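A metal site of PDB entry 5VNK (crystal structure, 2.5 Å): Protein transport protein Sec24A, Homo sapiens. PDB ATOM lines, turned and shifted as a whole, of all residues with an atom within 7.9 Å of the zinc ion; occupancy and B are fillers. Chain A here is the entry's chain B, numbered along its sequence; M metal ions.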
ATOM      1  N   ARG A  85     -22.087 -25.494  -4.225  1.00  0.00           N
ATOM      2  CA  ARG A  85     -21.687 -26.639  -5.025  1.00  0.00           C
ATOM      3  C   ARG A  85     -21.055 -26.147  -6.322  1.00  0.00           C
ATOM      4  O   ARG A  85     -21.236 -24.993  -6.727  1.00  0.00           O
ATOM      5  CB  ARG A  85     -22.875 -27.562  -5.338  1.00  0.00           C
ATOM      6  CG  ARG A  85     -23.638 -28.014  -4.105  1.00  0.00           C
ATOM      7  CD  ARG A  85     -24.750 -29.002  -4.456  1.00  0.00           C
ATOM      8  NE  ARG A  85     -24.232 -30.309  -4.838  1.00  0.00           N
ATOM      9  CZ  ARG A  85     -24.984 -31.405  -4.947  1.00  0.00           C
ATOM     10  NH1 ARG A  85     -26.292 -31.337  -4.699  1.00  0.00           N
ATOM     11  NH2 ARG A  85     -24.436 -32.558  -5.301  1.00  0.00           N
ATOM     12  N   CYS A  86     -20.288 -27.038  -6.964  1.00  0.00           N
ATOM     13  CA  CYS A  86     -19.689 -26.730  -8.254  1.00  0.00           C
ATOM     14  C   CYS A  86     -20.743 -26.794  -9.345  1.00  0.00           C
ATOM     15  O   CYS A  86     -21.539 -27.734  -9.405  1.00  0.00           O
ATOM     16  CB  CYS A  86     -18.550 -27.704  -8.561  1.00  0.00           C
ATOM     17  SG  CYS A  86     -17.850 -27.494 -10.224  1.00  0.00           S
ATOM     18  N   ARG A  87     -20.748 -25.786 -10.229  1.00  0.00           N
ATOM     19  CA  ARG A  87     -21.769 -25.699 -11.269  1.00  0.00           C
ATOM     20  C   ARG A  87     -21.665 -26.799 -12.306  1.00  0.00           C
ATOM     21  O   ARG A  87     -22.597 -26.953 -13.104  1.00  0.00           O
ATOM     22  CB  ARG A  87     -21.688 -24.334 -11.950  1.00  0.00           C
ATOM     23  CG  ARG A  87     -22.110 -23.161 -11.088  1.00  0.00           C
ATOM     24  CD  ARG A  87     -22.108 -21.866 -11.882  1.00  0.00           C
ATOM     25  NE  ARG A  87     -22.549 -20.718 -11.091  1.00  0.00           N
ATOM     26  CZ  ARG A  87     -22.588 -19.476 -11.539  1.00  0.00           C
ATOM     27  NH1 ARG A  87     -22.205 -19.210 -12.781  1.00  0.00           N
ATOM     28  NH2 ARG A  87     -23.006 -18.495 -10.752  1.00  0.00           N
ATOM     29  N   SER A  88     -20.579 -27.575 -12.328  1.00  0.00           N
ATOM     30  CA  SER A  88     -20.381 -28.616 -13.336  1.00  0.00           C
ATOM     31  C   SER A  88     -20.656 -30.008 -12.784  1.00  0.00           C
ATOM     32  O   SER A  88     -21.573 -30.700 -13.248  1.00  0.00           O
ATOM     33  CB  SER A  88     -18.966 -28.531 -13.908  1.00  0.00           C
ATOM     34  OG  SER A  88     -18.854 -27.473 -14.840  1.00  0.00           O
ATOM     35  N   CYS A  89     -19.863 -30.450 -11.800  1.00  0.00           N
ATOM     36  CA  CYS A  89     -19.968 -31.812 -11.277  1.00  0.00           C
ATOM     37  C   CYS A  89     -20.712 -31.881  -9.942  1.00  0.00           C
ATOM     38  O   CYS A  89     -20.720 -32.948  -9.315  1.00  0.00           O
ATOM     39  CB  CYS A  89     -18.572 -32.417 -11.138  1.00  0.00           C
ATOM     40  SG  CYS A  89     -17.504 -31.550  -9.958  1.00  0.00           S
ATOM     41  N   ARG A  90     -21.334 -30.784  -9.506  1.00  0.00           N
ATOM     42  CA  ARG A  90     -22.122 -30.721  -8.280  1.00  0.00           C
ATOM     43  C   ARG A  90     -21.307 -31.083  -7.037  1.00  0.00           C
ATOM     44  O   ARG A  90     -21.875 -31.482  -6.006  1.00  0.00           O
ATOM     45  CB  ARG A  90     -23.367 -31.613  -8.363  1.00  0.00           C
ATOM     46  CG  ARG A  90     -24.258 -31.351  -9.570  1.00  0.00           C
ATOM     47  CD  ARG A  90     -24.549 -29.866  -9.757  1.00  0.00           C
ATOM     48  NE  ARG A  90     -25.061 -29.246  -8.538  1.00  0.00           N
ATOM     49  CZ  ARG A  90     -26.341 -29.200  -8.201  1.00  0.00           C
ATOM     50  NH1 ARG A  90     -27.256 -29.750  -8.990  1.00  0.00           N
ATOM     51  NH2 ARG A  90     -26.714 -28.600  -7.077  1.00  0.00           N
ATOM     52  N   THR A  91     -19.985 -30.957  -7.099  1.00  0.00           N
ATOM     53  CA  THR A  91     -19.152 -31.213  -5.944  1.00  0.00           C
ATOM     54  C   THR A  91     -19.354 -30.140  -4.887  1.00  0.00           C
ATOM     55  O   THR A  91     -19.415 -28.948  -5.198  1.00  0.00           O
ATOM     56  CB  THR A  91     -17.677 -31.284  -6.348  1.00  0.00           C
ATOM     57  OG1 THR A  91     -17.498 -32.249  -7.380  1.00  0.00           O
ATOM     58  CG2 THR A  91     -16.812 -31.675  -5.154  1.00  0.00           C
ATOM     59  N   TYR A  92     -19.475 -30.568  -3.641  1.00  0.00           N
ATOM     60  CA  TYR A  92     -19.643 -29.623  -2.539  1.00  0.00           C
ATOM     61  C   TYR A  92     -18.330 -28.902  -2.266  1.00  0.00           C
ATOM     62  O   TYR A  92     -17.256 -29.508  -2.313  1.00  0.00           O
ATOM     63  CB  TYR A  92     -20.127 -30.346  -1.283  1.00  0.00           C
ATOM     64  CG  TYR A  92     -21.512 -30.931  -1.420  1.00  0.00           C
ATOM     65  CD1 TYR A  92     -21.711 -32.168  -2.009  1.00  0.00           C
ATOM     66  CD2 TYR A  92     -22.615 -30.233  -0.952  1.00  0.00           C
ATOM     67  CE1 TYR A  92     -22.986 -32.700  -2.136  1.00  0.00           C
ATOM     68  CE2 TYR A  92     -23.880 -30.760  -1.071  1.00  0.00           C
ATOM     69  CZ  TYR A  92     -24.064 -31.988  -1.661  1.00  0.00           C
ATOM     70  OH  TYR A  92     -25.327 -32.506  -1.775  1.00  0.00           O
ATOM     71  N   ASN A  94     -15.262 -27.595  -0.474  1.00  0.00           N
ATOM     72  CA  ASN A  94     -14.571 -28.460   0.466  1.00  0.00           C
ATOM     73  C   ASN A  94     -13.192 -27.851   0.747  1.00  0.00           C
ATOM     74  O   ASN A  94     -12.725 -27.000  -0.016  1.00  0.00           O
ATOM     75  CB  ASN A  94     -14.449 -29.881  -0.084  1.00  0.00           C
ATOM     76  CG  ASN A  94     -13.536 -29.974  -1.282  1.00  0.00           C
ATOM     77  OD1 ASN A  94     -12.345 -30.251  -1.149  1.00  0.00           O
ATOM     78  ND2 ASN A  94     -14.092 -29.759  -2.465  1.00  0.00           N
ATOM     79  N   TRP A 105     -13.649 -19.712  -6.938  1.00  0.00           N
ATOM     80  CA  TRP A 105     -12.966 -20.914  -6.468  1.00  0.00           C
ATOM     81  C   TRP A 105     -12.895 -21.945  -7.589  1.00  0.00           C
ATOM     82  O   TRP A 105     -13.789 -22.039  -8.424  1.00  0.00           O
ATOM     83  CB  TRP A 105     -13.664 -21.510  -5.231  1.00  0.00           C
ATOM     84  CG  TRP A 105     -15.097 -21.933  -5.429  1.00  0.00           C
ATOM     85  CD1 TRP A 105     -16.199 -21.129  -5.427  1.00  0.00           C
ATOM     86  CD2 TRP A 105     -15.582 -23.271  -5.642  1.00  0.00           C
ATOM     87  NE1 TRP A 105     -17.338 -21.873  -5.642  1.00  0.00           N
ATOM     88  CE2 TRP A 105     -16.981 -23.189  -5.770  1.00  0.00           C
ATOM     89  CE3 TRP A 105     -14.968 -24.523  -5.749  1.00  0.00           C
ATOM     90  CZ2 TRP A 105     -17.775 -24.317  -5.990  1.00  0.00           C
ATOM     91  CZ3 TRP A 105     -15.756 -25.639  -5.973  1.00  0.00           C
ATOM     92  CH2 TRP A 105     -17.145 -25.528  -6.093  1.00  0.00           C
ATOM     93  N   LYS A 106     -11.799 -22.704  -7.585  1.00  0.00           N
ATOM     94  CA  LYS A 106     -11.548 -23.723  -8.591  1.00  0.00           C
ATOM     95  C   LYS A 106     -11.853 -25.097  -7.997  1.00  0.00           C
ATOM     96  O   LYS A 106     -11.311 -25.449  -6.935  1.00  0.00           O
ATOM     97  CB  LYS A 106     -10.104 -23.673  -9.090  1.00  0.00           C
ATOM     98  CG  LYS A 106      -9.702 -24.847  -9.963  1.00  0.00           C
ATOM     99  CD  LYS A 106      -8.283 -24.710 -10.484  1.00  0.00           C
ATOM    100  CE  LYS A 106      -8.160 -23.604 -11.523  1.00  0.00           C
ATOM    101  NZ  LYS A 106      -6.802 -23.547 -12.126  1.00  0.00           N
ATOM    102  N   CYS A 107     -12.699 -25.855  -8.675  1.00  0.00           N
ATOM    103  CA  CYS A 107     -13.086 -27.169  -8.196  1.00  0.00           C
ATOM    104  C   CYS A 107     -11.891 -28.121  -8.217  1.00  0.00           C
ATOM    105  O   CYS A 107     -11.166 -28.198  -9.214  1.00  0.00           O
ATOM    106  CB  CYS A 107     -14.214 -27.722  -9.066  1.00  0.00           C
ATOM    107  SG  CYS A 107     -14.744 -29.365  -8.597  1.00  0.00           S
ATOM    108  N   ASN A 108     -11.686 -28.848  -7.119  1.00  0.00           N
ATOM    109  CA  ASN A 108     -10.588 -29.803  -7.059  1.00  0.00           C
ATOM    110  C   ASN A 108     -10.921 -31.135  -7.703  1.00  0.00           C
ATOM    111  O   ASN A 108     -10.077 -32.044  -7.673  1.00  0.00           O
ATOM    112  CB  ASN A 108     -10.154 -30.024  -5.600  1.00  0.00           C
ATOM    113  CG  ASN A 108     -11.324 -30.286  -4.671  1.00  0.00           C
ATOM    114  OD1 ASN A 108     -12.439 -29.807  -4.914  1.00  0.00           O
ATOM    115  ND2 ASN A 108     -11.079 -31.025  -3.606  1.00  0.00           N
ATOM    116  N   LEU A 109     -12.110 -31.291  -8.284  1.00  0.00           N
ATOM    117  CA  LEU A 109     -12.498 -32.516  -8.969  1.00  0.00           C
ATOM    118  C   LEU A 109     -12.718 -32.330 -10.465  1.00  0.00           C
ATOM    119  O   LEU A 109     -12.359 -33.222 -11.242  1.00  0.00           O
ATOM    120  CB  LEU A 109     -13.761 -33.116  -8.335  1.00  0.00           C
ATOM    121  CG  LEU A 109     -13.503 -34.070  -7.167  1.00  0.00           C
ATOM    122  CD1 LEU A 109     -13.211 -33.315  -5.881  1.00  0.00           C
ATOM    123  CD2 LEU A 109     -14.671 -35.023  -6.991  1.00  0.00           C
ATOM    124  N   CYS A 110     -13.308 -31.221 -10.891  1.00  0.00           N
ATOM    125  CA  CYS A 110     -13.501 -30.965 -12.314  1.00  0.00           C
ATOM    126  C   CYS A 110     -12.718 -29.770 -12.831  1.00  0.00           C
ATOM    127  O   CYS A 110     -12.754 -29.505 -14.042  1.00  0.00           O
ATOM    128  CB  CYS A 110     -15.001 -30.757 -12.622  1.00  0.00           C
ATOM    129  SG  CYS A 110     -15.752 -29.386 -11.722  1.00  0.00           S
ATOM    130  N   TYR A 111     -12.032 -29.019 -11.961  1.00  0.00           N
ATOM    131  CA  TYR A 111     -11.159 -27.885 -12.285  1.00  0.00           C
ATOM    132  C   TYR A 111     -11.907 -26.663 -12.806  1.00  0.00           C
ATOM    133  O   TYR A 111     -11.270 -25.674 -13.179  1.00  0.00           O
ATOM    134  CB  TYR A 111     -10.066 -28.272 -13.302  1.00  0.00           C
ATOM    135  CG  TYR A 111      -9.306 -29.527 -12.950  1.00  0.00           C
ATOM    136  CD1 TYR A 111      -8.894 -29.769 -11.648  1.00  0.00           C
ATOM    137  CD2 TYR A 111      -9.013 -30.469 -13.921  1.00  0.00           C
ATOM    138  CE1 TYR A 111      -8.209 -30.930 -11.330  1.00  0.00           C
ATOM    139  CE2 TYR A 111      -8.336 -31.626 -13.606  1.00  0.00           C
ATOM    140  CZ  TYR A 111      -7.927 -31.853 -12.310  1.00  0.00           C
ATOM    141  OH  TYR A 111      -7.244 -33.011 -12.016  1.00  0.00           O
ATOM    142  N   ARG A 112     -13.238 -26.696 -12.840  1.00  0.00           N
ATOM    143  CA  ARG A 112     -13.987 -25.542 -13.307  1.00  0.00           C
ATOM    144  C   ARG A 112     -13.985 -24.441 -12.249  1.00  0.00           C
ATOM    145  O   ARG A 112     -14.098 -24.700 -11.055  1.00  0.00           O
ATOM    146  CB  ARG A 112     -15.424 -25.935 -13.654  1.00  0.00           C
ATOM    147  CG  ARG A 112     -16.414 -24.796 -13.483  1.00  0.00           C
ATOM    148  CD  ARG A 112     -17.452 -24.725 -14.589  1.00  0.00           C
ATOM    149  NE  ARG A 112     -18.283 -23.537 -14.458  1.00  0.00           N
ATOM    150  CZ  ARG A 112     -19.560 -23.483 -14.803  1.00  0.00           C
ATOM    151  NH1 ARG A 112     -20.161 -24.557 -15.287  1.00  0.00           N
ATOM    152  NH2 ARG A 112     -20.245 -22.362 -14.648  1.00  0.00           N
ATOM    153  N   VAL A 113     -13.857 -23.198 -12.717  1.00  0.00           N
ATOM    154  CA  VAL A 113     -13.875 -22.042 -11.828  1.00  0.00           C
ATOM    155  C   VAL A 113     -15.320 -21.634 -11.570  1.00  0.00           C
ATOM    156  O   VAL A 113     -16.147 -21.602 -12.482  1.00  0.00           O
ATOM    157  CB  VAL A 113     -13.070 -20.885 -12.449  1.00  0.00           C
ATOM    158  CG1 VAL A 113     -12.869 -19.771 -11.425  1.00  0.00           C
ATOM    159  CG2 VAL A 113     -11.739 -21.389 -12.986  1.00  0.00           C
ATOM    160  N   ASN A 114     -15.626 -21.331 -10.303  1.00  0.00           N
ATOM    161  CA  ASN A 114     -16.984 -21.013  -9.880  1.00  0.00           C
ATOM    162  C   ASN A 114     -17.011 -19.660  -9.187  1.00  0.00           C
ATOM    163  O   ASN A 114     -15.983 -19.081  -8.851  1.00  0.00           O
ATOM    164  CB  ASN A 114     -17.544 -22.092  -8.954  1.00  0.00           C
ATOM    165  CG  ASN A 114     -17.847 -23.394  -9.679  1.00  0.00           C
ATOM    166  OD1 ASN A 114     -19.003 -23.720  -9.940  1.00  0.00           O
ATOM    167  ND2 ASN A 114     -16.793 -24.131 -10.020  1.00  0.00           N
ATOM    168  N   ARG A 407     -17.549 -39.330  -5.425  1.00  0.00           N
ATOM    169  CA  ARG A 407     -16.910 -38.595  -6.494  1.00  0.00           C
ATOM    170  C   ARG A 407     -15.405 -38.584  -6.302  1.00  0.00           C
ATOM    171  O   ARG A 407     -14.904 -38.591  -5.173  1.00  0.00           O
ATOM    172  CB  ARG A 407     -17.408 -37.143  -6.550  1.00  0.00           C
ATOM    173  CG  ARG A 407     -18.834 -36.950  -7.021  1.00  0.00           C
ATOM    174  CD  ARG A 407     -19.133 -35.462  -7.150  1.00  0.00           C
ATOM    175  NE  ARG A 407     -20.531 -35.176  -7.428  1.00  0.00           N
ATOM    176  CZ  ARG A 407     -21.470 -35.065  -6.494  1.00  0.00           C
ATOM    177  NH1 ARG A 407     -21.158 -35.238  -5.214  1.00  0.00           N
ATOM    178  NH2 ARG A 407     -22.718 -34.797  -6.834  1.00  0.00           N
HETATM  179 ZN    ZN M   1     -16.774 -29.416  -9.706  1.00  0.00          ZN
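The side-chain sulfur of Cys 107 sits close to the backbone NH of Leu 109, 3.3 Å away.
The side-chain sulfur (SG) of Cys 89 lies close to the side-chain hydroxyl (OG1) of Thr 91, 2.7 Å away.
The backbone carbonyl oxygen (O) of Arg 112 is in hydrogen-bond range of the backbone NH (N) of Cys 107 (3.0 Å).
The side-chain sulfur (SG) of Cys 86 lies close to the backbone NH (N) of Ser 88 (3.4 Å).
The backbone carbonyl oxygen (O) of Cys 89 lies within hydrogen-bond range of the guanidinium group (NE) of Arg 407.
The backbone NH (N) of Cys 86 sits at hydrogen-bond distance from the backbone carbonyl oxygen (O) of Thr 91, 2.7 Å away.
ND2 of Asn 114 sits close to SG of Cys 86 (3.5 Å).
OG1 of Thr 91 touches the zinc ion, at 3.7 Å.
The nearest printed residue that does not touch the zinc ion is Arg 90 (4.8 Å).
The side-chain sulfur (SG) of Cys 110 binds the zinc ion.
SG of Cys 86 binds the zinc ion (2.3 Å).
The zinc ion is bound by SG of Cys 89 (2.3 Å).
SG of Cys 107 is bound to the zinc ion.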
